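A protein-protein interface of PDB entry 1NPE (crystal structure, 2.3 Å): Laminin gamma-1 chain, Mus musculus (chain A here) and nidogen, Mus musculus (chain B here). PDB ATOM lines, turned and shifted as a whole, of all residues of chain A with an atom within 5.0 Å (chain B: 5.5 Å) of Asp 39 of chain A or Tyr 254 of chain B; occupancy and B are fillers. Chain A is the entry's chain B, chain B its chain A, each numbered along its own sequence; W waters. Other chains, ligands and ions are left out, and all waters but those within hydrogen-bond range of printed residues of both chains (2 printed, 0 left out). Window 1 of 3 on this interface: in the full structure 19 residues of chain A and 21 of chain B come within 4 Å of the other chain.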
ATOM      1  N   CYS A  37       6.337 -15.199 -21.399  1.00  0.00           N
ATOM      2  CA  CYS A  37       6.615 -14.488 -20.165  1.00  0.00           C
ATOM      3  C   CYS A  37       6.797 -15.460 -19.022  1.00  0.00           C
ATOM      4  O   CYS A  37       6.164 -16.517 -18.972  1.00  0.00           O
ATOM      5  CB  CYS A  37       5.497 -13.504 -19.814  1.00  0.00           C
ATOM      6  SG  CYS A  37       5.185 -12.244 -21.082  1.00  0.00           S
ATOM      7  N   ASP A  38       7.662 -15.071 -18.098  1.00  0.00           N
ATOM      8  CA  ASP A  38       7.958 -15.856 -16.920  1.00  0.00           C
ATOM      9  C   ASP A  38       6.757 -15.746 -15.987  1.00  0.00           C
ATOM     10  O   ASP A  38       5.950 -14.815 -16.112  1.00  0.00           O
ATOM     11  CB  ASP A  38       9.207 -15.276 -16.242  1.00  0.00           C
ATOM     12  CG  ASP A  38       9.871 -16.252 -15.291  1.00  0.00           C
ATOM     13  OD1 ASP A  38       9.559 -17.458 -15.356  1.00  0.00           O
ATOM     14  OD2 ASP A  38      10.721 -15.810 -14.484  1.00  0.00           O
ATOM     15  N   ASP A  39       6.610 -16.710 -15.081  1.00  0.00           N
ATOM     16  CA  ASP A  39       5.513 -16.661 -14.128  1.00  0.00           C
ATOM     17  C   ASP A  39       5.703 -15.376 -13.339  1.00  0.00           C
ATOM     18  O   ASP A  39       6.825 -15.051 -12.948  1.00  0.00           O
ATOM     19  CB  ASP A  39       5.544 -17.856 -13.175  1.00  0.00           C
ATOM     20  CG  ASP A  39       4.463 -17.773 -12.116  1.00  0.00           C
ATOM     21  OD1 ASP A  39       3.268 -17.836 -12.469  1.00  0.00           O
ATOM     22  OD2 ASP A  39       4.810 -17.611 -10.936  1.00  0.00           O
ATOM     23  N   GLY A  40       4.608 -14.650 -13.126  1.00  0.00           N
ATOM     24  CA  GLY A  40       4.662 -13.384 -12.407  1.00  0.00           C
ATOM     25  C   GLY A  40       4.590 -12.212 -13.379  1.00  0.00           C
ATOM     26  O   GLY A  40       4.535 -11.055 -12.969  1.00  0.00           O
ATOM     27  N   TYR A  41       4.595 -12.528 -14.674  1.00  0.00           N
ATOM     28  CA  TYR A  41       4.534 -11.541 -15.750  1.00  0.00           C
ATOM     29  C   TYR A  41       3.467 -11.971 -16.746  1.00  0.00           C
ATOM     30  O   TYR A  41       2.991 -13.110 -16.710  1.00  0.00           O
ATOM     31  CB  TYR A  41       5.881 -11.450 -16.494  1.00  0.00           C
ATOM     32  CG  TYR A  41       7.038 -10.896 -15.683  1.00  0.00           C
ATOM     33  CD1 TYR A  41       7.681 -11.679 -14.717  1.00  0.00           C
ATOM     34  CD2 TYR A  41       7.482  -9.586 -15.879  1.00  0.00           C
ATOM     35  CE1 TYR A  41       8.736 -11.169 -13.959  1.00  0.00           C
ATOM     36  CE2 TYR A  41       8.531  -9.063 -15.130  1.00  0.00           C
ATOM     37  CZ  TYR A  41       9.152  -9.857 -14.167  1.00  0.00           C
ATOM     38  OH  TYR A  41      10.167  -9.328 -13.397  1.00  0.00           O
ATOM     39  N   ALA A  68       3.206 -16.141  -3.727  1.00  0.00           N
ATOM     40  CA  ALA A  68       2.421 -17.112  -4.479  1.00  0.00           C
ATOM     41  C   ALA A  68       2.957 -17.224  -5.899  1.00  0.00           C
ATOM     42  O   ALA A  68       3.685 -16.349  -6.362  1.00  0.00           O
ATOM     43  CB  ALA A  68       0.956 -16.692  -4.513  1.00  0.00           C
ATOM     44  N   VAL A  69       2.634 -18.331  -6.560  1.00  0.00           N
ATOM     45  CA  VAL A  69       3.025 -18.560  -7.948  1.00  0.00           C
ATOM     46  C   VAL A  69       1.716 -18.608  -8.741  1.00  0.00           C
ATOM     47  O   VAL A  69       0.661 -18.879  -8.167  1.00  0.00           O
ATOM     48  CB  VAL A  69       3.791 -19.906  -8.130  1.00  0.00           C
ATOM     49  CG1 VAL A  69       5.168 -19.814  -7.506  1.00  0.00           C
ATOM     50  CG2 VAL A  69       3.007 -21.071  -7.507  1.00  0.00           C
ATOM     51  N   GLY A  70       1.774 -18.338 -10.044  1.00  0.00           N
ATOM     52  CA  GLY A  70       0.565 -18.359 -10.858  1.00  0.00           C
ATOM     53  C   GLY A  70      -0.430 -17.266 -10.484  1.00  0.00           C
ATOM     54  O   GLY A  70      -1.646 -17.468 -10.537  1.00  0.00           O
ATOM     55  N   ASN A  71       0.092 -16.110 -10.087  1.00  0.00           N
ATOM     56  CA  ASN A  71      -0.735 -14.976  -9.709  1.00  0.00           C
ATOM     57  C   ASN A  71      -1.610 -14.423 -10.830  1.00  0.00           C
ATOM     58  O   ASN A  71      -2.709 -13.953 -10.558  1.00  0.00           O
ATOM     59  CB  ASN A  71       0.115 -13.875  -9.091  1.00  0.00           C
ATOM     60  CG  ASN A  71       0.336 -14.091  -7.614  1.00  0.00           C
ATOM     61  OD1 ASN A  71      -0.506 -14.688  -6.934  1.00  0.00           O
ATOM     62  ND2 ASN A  71       1.470 -13.623  -7.102  1.00  0.00           N
ATOM     63  N   ARG A  74      -0.424 -15.600 -17.899  1.00  0.00           N
ATOM     64  CA  ARG A  74       0.759 -15.095 -18.602  1.00  0.00           C
ATOM     65  C   ARG A  74       0.564 -14.468 -19.985  1.00  0.00           C
ATOM     66  O   ARG A  74       1.486 -13.852 -20.523  1.00  0.00           O
ATOM     67  CB  ARG A  74       1.848 -16.175 -18.650  1.00  0.00           C
ATOM     68  CG  ARG A  74       2.404 -16.499 -17.273  1.00  0.00           C
ATOM     69  CD  ARG A  74       3.510 -17.521 -17.314  1.00  0.00           C
ATOM     70  NE  ARG A  74       3.075 -18.780 -17.905  1.00  0.00           N
ATOM     71  CZ  ARG A  74       3.780 -19.456 -18.804  1.00  0.00           C
ATOM     72  NH1 ARG A  74       4.955 -18.991 -19.219  1.00  0.00           N
ATOM     73  NH2 ARG A  74       3.323 -20.609 -19.269  1.00  0.00           N
ATOM     74  N   PHE B   6      16.465 -29.048 -10.992  1.00  0.00           N
ATOM     75  CA  PHE B   6      15.663 -27.911 -10.561  1.00  0.00           C
ATOM     76  C   PHE B   6      14.715 -27.405 -11.643  1.00  0.00           C
ATOM     77  O   PHE B   6      14.931 -27.632 -12.830  1.00  0.00           O
ATOM     78  CB  PHE B   6      16.514 -26.786  -9.955  1.00  0.00           C
ATOM     79  CG  PHE B   6      17.445 -26.112 -10.924  1.00  0.00           C
ATOM     80  CD1 PHE B   6      18.788 -26.481 -10.987  1.00  0.00           C
ATOM     81  CD2 PHE B   6      16.998 -25.061 -11.719  1.00  0.00           C
ATOM     82  CE1 PHE B   6      19.682 -25.809 -11.823  1.00  0.00           C
ATOM     83  CE2 PHE B   6      17.879 -24.380 -12.558  1.00  0.00           C
ATOM     84  CZ  PHE B   6      19.230 -24.756 -12.607  1.00  0.00           C
ATOM     85  N   ALA B   7      13.649 -26.738 -11.217  1.00  0.00           N
ATOM     86  CA  ALA B   7      12.642 -26.234 -12.132  1.00  0.00           C
ATOM     87  C   ALA B   7      12.711 -24.747 -12.461  1.00  0.00           C
ATOM     88  O   ALA B   7      13.108 -23.924 -11.637  1.00  0.00           O
ATOM     89  CB  ALA B   7      11.257 -26.578 -11.604  1.00  0.00           C
ATOM     90  N   GLN B   8      12.324 -24.437 -13.695  1.00  0.00           N
ATOM     91  CA  GLN B   8      12.244 -23.079 -14.224  1.00  0.00           C
ATOM     92  C   GLN B   8      11.026 -23.086 -15.132  1.00  0.00           C
ATOM     93  O   GLN B   8      10.474 -24.153 -15.425  1.00  0.00           O
ATOM     94  CB  GLN B   8      13.482 -22.709 -15.043  1.00  0.00           C
ATOM     95  CG  GLN B   8      14.599 -22.075 -14.237  1.00  0.00           C
ATOM     96  CD  GLN B   8      15.817 -21.727 -15.080  1.00  0.00           C
ATOM     97  OE1 GLN B   8      16.261 -22.522 -15.904  1.00  0.00           O
ATOM     98  NE2 GLN B   8      16.370 -20.541 -14.863  1.00  0.00           N
ATOM     99  N   THR B   9      10.579 -21.903 -15.543  1.00  0.00           N
ATOM    100  CA  THR B   9       9.426 -21.805 -16.424  1.00  0.00           C
ATOM    101  C   THR B   9       9.794 -22.446 -17.751  1.00  0.00           C
ATOM    102  O   THR B   9      10.819 -22.113 -18.345  1.00  0.00           O
ATOM    103  CB  THR B   9       8.998 -20.334 -16.640  1.00  0.00           C
ATOM    104  OG1 THR B   9       8.536 -19.782 -15.401  1.00  0.00           O
ATOM    105  CG2 THR B   9       7.887 -20.228 -17.669  1.00  0.00           C
ATOM    106  N   VAL B  37       4.773 -24.352 -16.407  1.00  0.00           N
ATOM    107  CA  VAL B  37       5.487 -23.657 -15.344  1.00  0.00           C
ATOM    108  C   VAL B  37       5.662 -24.743 -14.281  1.00  0.00           C
ATOM    109  O   VAL B  37       4.759 -25.001 -13.476  1.00  0.00           O
ATOM    110  CB  VAL B  37       4.688 -22.456 -14.768  1.00  0.00           C
ATOM    111  CG1 VAL B  37       5.410 -21.875 -13.560  1.00  0.00           C
ATOM    112  CG2 VAL B  37       4.504 -21.377 -15.833  1.00  0.00           C
ATOM    113  N   ILE B  38       6.792 -25.440 -14.358  1.00  0.00           N
ATOM    114  CA  ILE B  38       7.112 -26.521 -13.439  1.00  0.00           C
ATOM    115  C   ILE B  38       7.401 -25.946 -12.058  1.00  0.00           C
ATOM    116  O   ILE B  38       8.226 -25.046 -11.917  1.00  0.00           O
ATOM    117  CB  ILE B  38       8.351 -27.308 -13.925  1.00  0.00           C
ATOM    118  CG1 ILE B  38       8.212 -27.669 -15.407  1.00  0.00           C
ATOM    119  CG2 ILE B  38       8.518 -28.580 -13.103  1.00  0.00           C
ATOM    120  CD1 ILE B  38       7.193 -28.757 -15.697  1.00  0.00           C
ATOM    121  N   ILE B  39       6.724 -26.465 -11.040  1.00  0.00           N
ATOM    122  CA  ILE B  39       6.921 -25.971  -9.684  1.00  0.00           C
ATOM    123  C   ILE B  39       7.560 -27.007  -8.763  1.00  0.00           C
ATOM    124  O   ILE B  39       8.683 -26.812  -8.302  1.00  0.00           O
ATOM    125  CB  ILE B  39       5.598 -25.477  -9.070  1.00  0.00           C
ATOM    126  CG1 ILE B  39       4.991 -24.369  -9.940  1.00  0.00           C
ATOM    127  CG2 ILE B  39       5.832 -24.973  -7.652  1.00  0.00           C
ATOM    128  CD1 ILE B  39       5.790 -23.069  -9.947  1.00  0.00           C
ATOM    129  N   ILE B  55       1.644 -25.755 -12.637  1.00  0.00           N
ATOM    130  CA  ILE B  55       0.537 -24.867 -12.270  1.00  0.00           C
ATOM    131  C   ILE B  55      -0.115 -24.180 -13.470  1.00  0.00           C
ATOM    132  O   ILE B  55      -1.088 -23.441 -13.311  1.00  0.00           O
ATOM    133  CB  ILE B  55       0.989 -23.756 -11.312  1.00  0.00           C
ATOM    134  CG1 ILE B  55       2.168 -22.995 -11.927  1.00  0.00           C
ATOM    135  CG2 ILE B  55       1.308 -24.333  -9.949  1.00  0.00           C
ATOM    136  CD1 ILE B  55       2.475 -21.693 -11.243  1.00  0.00           C
ATOM    137  N   PHE B 212      12.930 -20.665  -2.017  1.00  0.00           N
ATOM    138  CA  PHE B 212      11.663 -21.208  -2.476  1.00  0.00           C
ATOM    139  C   PHE B 212      11.558 -22.707  -2.193  1.00  0.00           C
ATOM    140  O   PHE B 212      10.534 -23.179  -1.702  1.00  0.00           O
ATOM    141  CB  PHE B 212      11.438 -20.977  -3.969  1.00  0.00           C
ATOM    142  CG  PHE B 212      10.180 -21.612  -4.469  1.00  0.00           C
ATOM    143  CD1 PHE B 212       8.952 -20.983  -4.281  1.00  0.00           C
ATOM    144  CD2 PHE B 212      10.201 -22.890  -5.036  1.00  0.00           C
ATOM    145  CE1 PHE B 212       7.766 -21.613  -4.639  1.00  0.00           C
ATOM    146  CE2 PHE B 212       9.023 -23.524  -5.396  1.00  0.00           C
ATOM    147  CZ  PHE B 212       7.800 -22.886  -5.195  1.00  0.00           C
ATOM    148  N   ALA B 213      12.579 -23.463  -2.592  1.00  0.00           N
ATOM    149  CA  ALA B 213      12.578 -24.902  -2.381  1.00  0.00           C
ATOM    150  C   ALA B 213      13.929 -25.361  -1.873  1.00  0.00           C
ATOM    151  O   ALA B 213      14.934 -24.662  -2.022  1.00  0.00           O
ATOM    152  CB  ALA B 213      12.226 -25.631  -3.665  1.00  0.00           C
ATOM    153  N   THR B 224      16.744 -23.151  -3.817  1.00  0.00           N
ATOM    154  CA  THR B 224      16.542 -22.232  -4.930  1.00  0.00           C
ATOM    155  C   THR B 224      16.140 -20.894  -4.337  1.00  0.00           C
ATOM    156  O   THR B 224      15.337 -20.840  -3.398  1.00  0.00           O
ATOM    157  CB  THR B 224      15.450 -22.727  -5.889  1.00  0.00           C
ATOM    158  OG1 THR B 224      14.214 -22.882  -5.178  1.00  0.00           O
ATOM    159  CG2 THR B 224      15.865 -24.061  -6.520  1.00  0.00           C
ATOM    160  N   TRP B 226      14.774 -16.893  -5.139  1.00  0.00           N
ATOM    161  CA  TRP B 226      14.089 -15.967  -6.047  1.00  0.00           C
ATOM    162  C   TRP B 226      14.766 -14.593  -6.176  1.00  0.00           C
ATOM    163  O   TRP B 226      14.612 -13.903  -7.187  1.00  0.00           O
ATOM    164  CB  TRP B 226      12.650 -15.764  -5.572  1.00  0.00           C
ATOM    165  CG  TRP B 226      11.709 -16.879  -5.921  1.00  0.00           C
ATOM    166  CD1 TRP B 226      12.014 -18.063  -6.537  1.00  0.00           C
ATOM    167  CD2 TRP B 226      10.295 -16.889  -5.711  1.00  0.00           C
ATOM    168  NE1 TRP B 226      10.875 -18.805  -6.722  1.00  0.00           N
ATOM    169  CE2 TRP B 226       9.806 -18.108  -6.225  1.00  0.00           C
ATOM    170  CE3 TRP B 226       9.392 -15.985  -5.134  1.00  0.00           C
ATOM    171  CZ2 TRP B 226       8.454 -18.446  -6.181  1.00  0.00           C
ATOM    172  CZ3 TRP B 226       8.051 -16.323  -5.089  1.00  0.00           C
ATOM    173  CH2 TRP B 226       7.594 -17.547  -5.610  1.00  0.00           C
ATOM    174  N   ARG B 252      12.928 -17.229 -13.015  1.00  0.00           N
ATOM    175  CA  ARG B 252      12.552 -17.721 -11.688  1.00  0.00           C
ATOM    176  C   ARG B 252      12.782 -19.229 -11.490  1.00  0.00           C
ATOM    177  O   ARG B 252      12.283 -20.051 -12.258  1.00  0.00           O
ATOM    178  CB  ARG B 252      11.081 -17.396 -11.427  1.00  0.00           C
ATOM    179  CG  ARG B 252      10.697 -17.273  -9.965  1.00  0.00           C
ATOM    180  CD  ARG B 252      11.182 -15.967  -9.397  1.00  0.00           C
ATOM    181  NE  ARG B 252      10.101 -15.181  -8.814  1.00  0.00           N
ATOM    182  CZ  ARG B 252      10.260 -13.969  -8.289  1.00  0.00           C
ATOM    183  NH1 ARG B 252      11.459 -13.400  -8.269  1.00  0.00           N
ATOM    184  NH2 ARG B 252       9.220 -13.323  -7.785  1.00  0.00           N
ATOM    185  N   LEU B 253      13.569 -19.573 -10.479  1.00  0.00           N
ATOM    186  CA  LEU B 253      13.847 -20.968 -10.152  1.00  0.00           C
ATOM    187  C   LEU B 253      12.765 -21.490  -9.207  1.00  0.00           C
ATOM    188  O   LEU B 253      12.316 -20.762  -8.330  1.00  0.00           O
ATOM    189  CB  LEU B 253      15.203 -21.092  -9.453  1.00  0.00           C
ATOM    190  CG  LEU B 253      16.472 -20.677 -10.200  1.00  0.00           C
ATOM    191  CD1 LEU B 253      17.668 -21.127  -9.392  1.00  0.00           C
ATOM    192  CD2 LEU B 253      16.515 -21.336 -11.555  1.00  0.00           C
ATOM    193  N   TYR B 254      12.362 -22.748  -9.368  1.00  0.00           N
ATOM    194  CA  TYR B 254      11.346 -23.317  -8.495  1.00  0.00           C
ATOM    195  C   TYR B 254      11.810 -24.546  -7.702  1.00  0.00           C
ATOM    196  O   TYR B 254      12.785 -24.464  -6.957  1.00  0.00           O
ATOM    197  CB  TYR B 254      10.055 -23.580  -9.279  1.00  0.00           C
ATOM    198  CG  TYR B 254       9.459 -22.301  -9.831  1.00  0.00           C
ATOM    199  CD1 TYR B 254       8.946 -21.324  -8.973  1.00  0.00           C
ATOM    200  CD2 TYR B 254       9.465 -22.033 -11.203  1.00  0.00           C
ATOM    201  CE1 TYR B 254       8.461 -20.112  -9.463  1.00  0.00           C
ATOM    202  CE2 TYR B 254       8.980 -20.821 -11.705  1.00  0.00           C
ATOM    203  CZ  TYR B 254       8.485 -19.867 -10.830  1.00  0.00           C
ATOM    204  OH  TYR B 254       8.051 -18.652 -11.306  1.00  0.00           O
ATOM    205  N   GLY B 255      11.101 -25.663  -7.841  1.00  0.00           N
ATOM    206  CA  GLY B 255      11.451 -26.872  -7.117  1.00  0.00           C
ATOM    207  C   GLY B 255      12.847 -27.402  -7.381  1.00  0.00           C
ATOM    208  O   GLY B 255      13.459 -27.110  -8.410  1.00  0.00           O
ATOM    209  N   ILE B 256      13.332 -28.214  -6.453  1.00  0.00           N
ATOM    210  CA  ILE B 256      14.657 -28.800  -6.554  1.00  0.00           C
ATOM    211  C   ILE B 256      14.653 -30.172  -5.887  1.00  0.00           C
ATOM    212  O   ILE B 256      14.037 -30.363  -4.837  1.00  0.00           O
ATOM    213  CB  ILE B 256      15.720 -27.878  -5.896  1.00  0.00           C
ATOM    214  CG1 ILE B 256      17.132 -28.352  -6.225  1.00  0.00           C
ATOM    215  CG2 ILE B 256      15.512 -27.804  -4.398  1.00  0.00           C
ATOM    216  CD1 ILE B 256      18.202 -27.341  -5.845  1.00  0.00           C
HETATM  217  O   HOH W   1      11.495 -19.265 -14.679  1.00  0.00           O
HETATM  218  O   HOH W   2       6.703 -16.179  -9.555  1.00  0.00           O
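OG1 of Thr 9 of chain B sits at hydrogen-bond distance from OD1 of Asp 38 of chain A. The side-chain carboxylate (OD2) of Asp 38 of chain A is in hydrogen-bond range of the backbone NH (N) of Arg 252 of chain B (3.0 Å). OH of Tyr 254 of chain B sits close to OD2 of Asp 39 of chain A (3.4 Å).
The backbone carbonyl oxygen (O) of Leu 253 of chain B is in hydrogen-bond range of the indole nitrogen (NE1) of Trp 226 of chain B, at 2.9 Å. O of Cys 37 of chain A is in hydrogen-bond range of NH1 of Arg 74 of chain A, at 2.8 Å. The backbone NH (N) of Ile 55 of chain B lies within hydrogen-bond range of the backbone carbonyl oxygen (O) of Val 37 of chain B. N of Tyr 254 of chain B sits at hydrogen-bond distance from O of Ala 7 of chain B, 2.7 Å away. The backbone carbonyl oxygen of Trp 226 of chain B is in hydrogen-bond range of the guanidinium group of Arg 252 of chain B (3.4 Å). OD1 of Asp 39 of chain A is in hydrogen-bond range of N of Gly 70 of chain A (2.9 Å).
OG1 of Thr 9 of chain B touches N of Asp 39 of chain A (3.6 Å). Val 69 of chain A touches Ile 55 of chain B (CB to CD1, 3.8 Å). Val 69 of chain A touches Trp 226 of chain B. Tyr 254 of chain B touches Val 69 of chain A (CE1 to CG1, 3.8 Å). Ile 55 of chain B touches Gly 70 of chain A. NH1 of Arg 74 of chain A touches CG2 of Thr 9 of chain B, at 3.5 Å. Val 37 of chain B touches Arg 74 of chain A.
Asp 39 of chain A touches just these residues of chain B: Thr 9 and Tyr 254. Of chain A, only Asp 39 and Val 69 come within 4 Å of Tyr 254 of chain B. Of the printed residues of chain B, Val 69 of chain A touches Ile 55 (3.8 Å), Trp 226 (3.8 Å) and Tyr 254 (3.8 Å). Printed residues of chain B within 4 Å of Arg 74 of chain A: Thr 9 (3.5 Å) and Val 37 (3.6 Å). Ala 213 of chain B touches none of the printed residues of chain A. The nearest residue of chain A that does not touch Tyr 254 of chain B is Asp 38 of chain A (4.5 Å).
Printed residues of chain B that touch a printed residue of chain A: Thr 9, Val 37, Ile 55, Trp 226, Arg 252 and Tyr 254. Hydrophobic or aromatic side chains of chain B within 4 Å of the printed part of chain A: Val 37, Ile 55, Trp 226 and Tyr 254. Among the printed residues, 10 pairs touch across the chains. Among the printed residues, no Asp or Glu carboxylate lies within 4 Å of a Lys or Arg side-chain nitrogen of the other chain.
Water W1 lies within hydrogen-bond range of O of Arg 252 of chain B, OD1 of Asp 38 of chain A and N of Thr 9 of chain B. Water W2 lies within hydrogen-bond range of the side-chain carboxylate (OD2) of Asp 39 of chain A and the side-chain hydroxyl (OH) of Tyr 254 of chain B.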
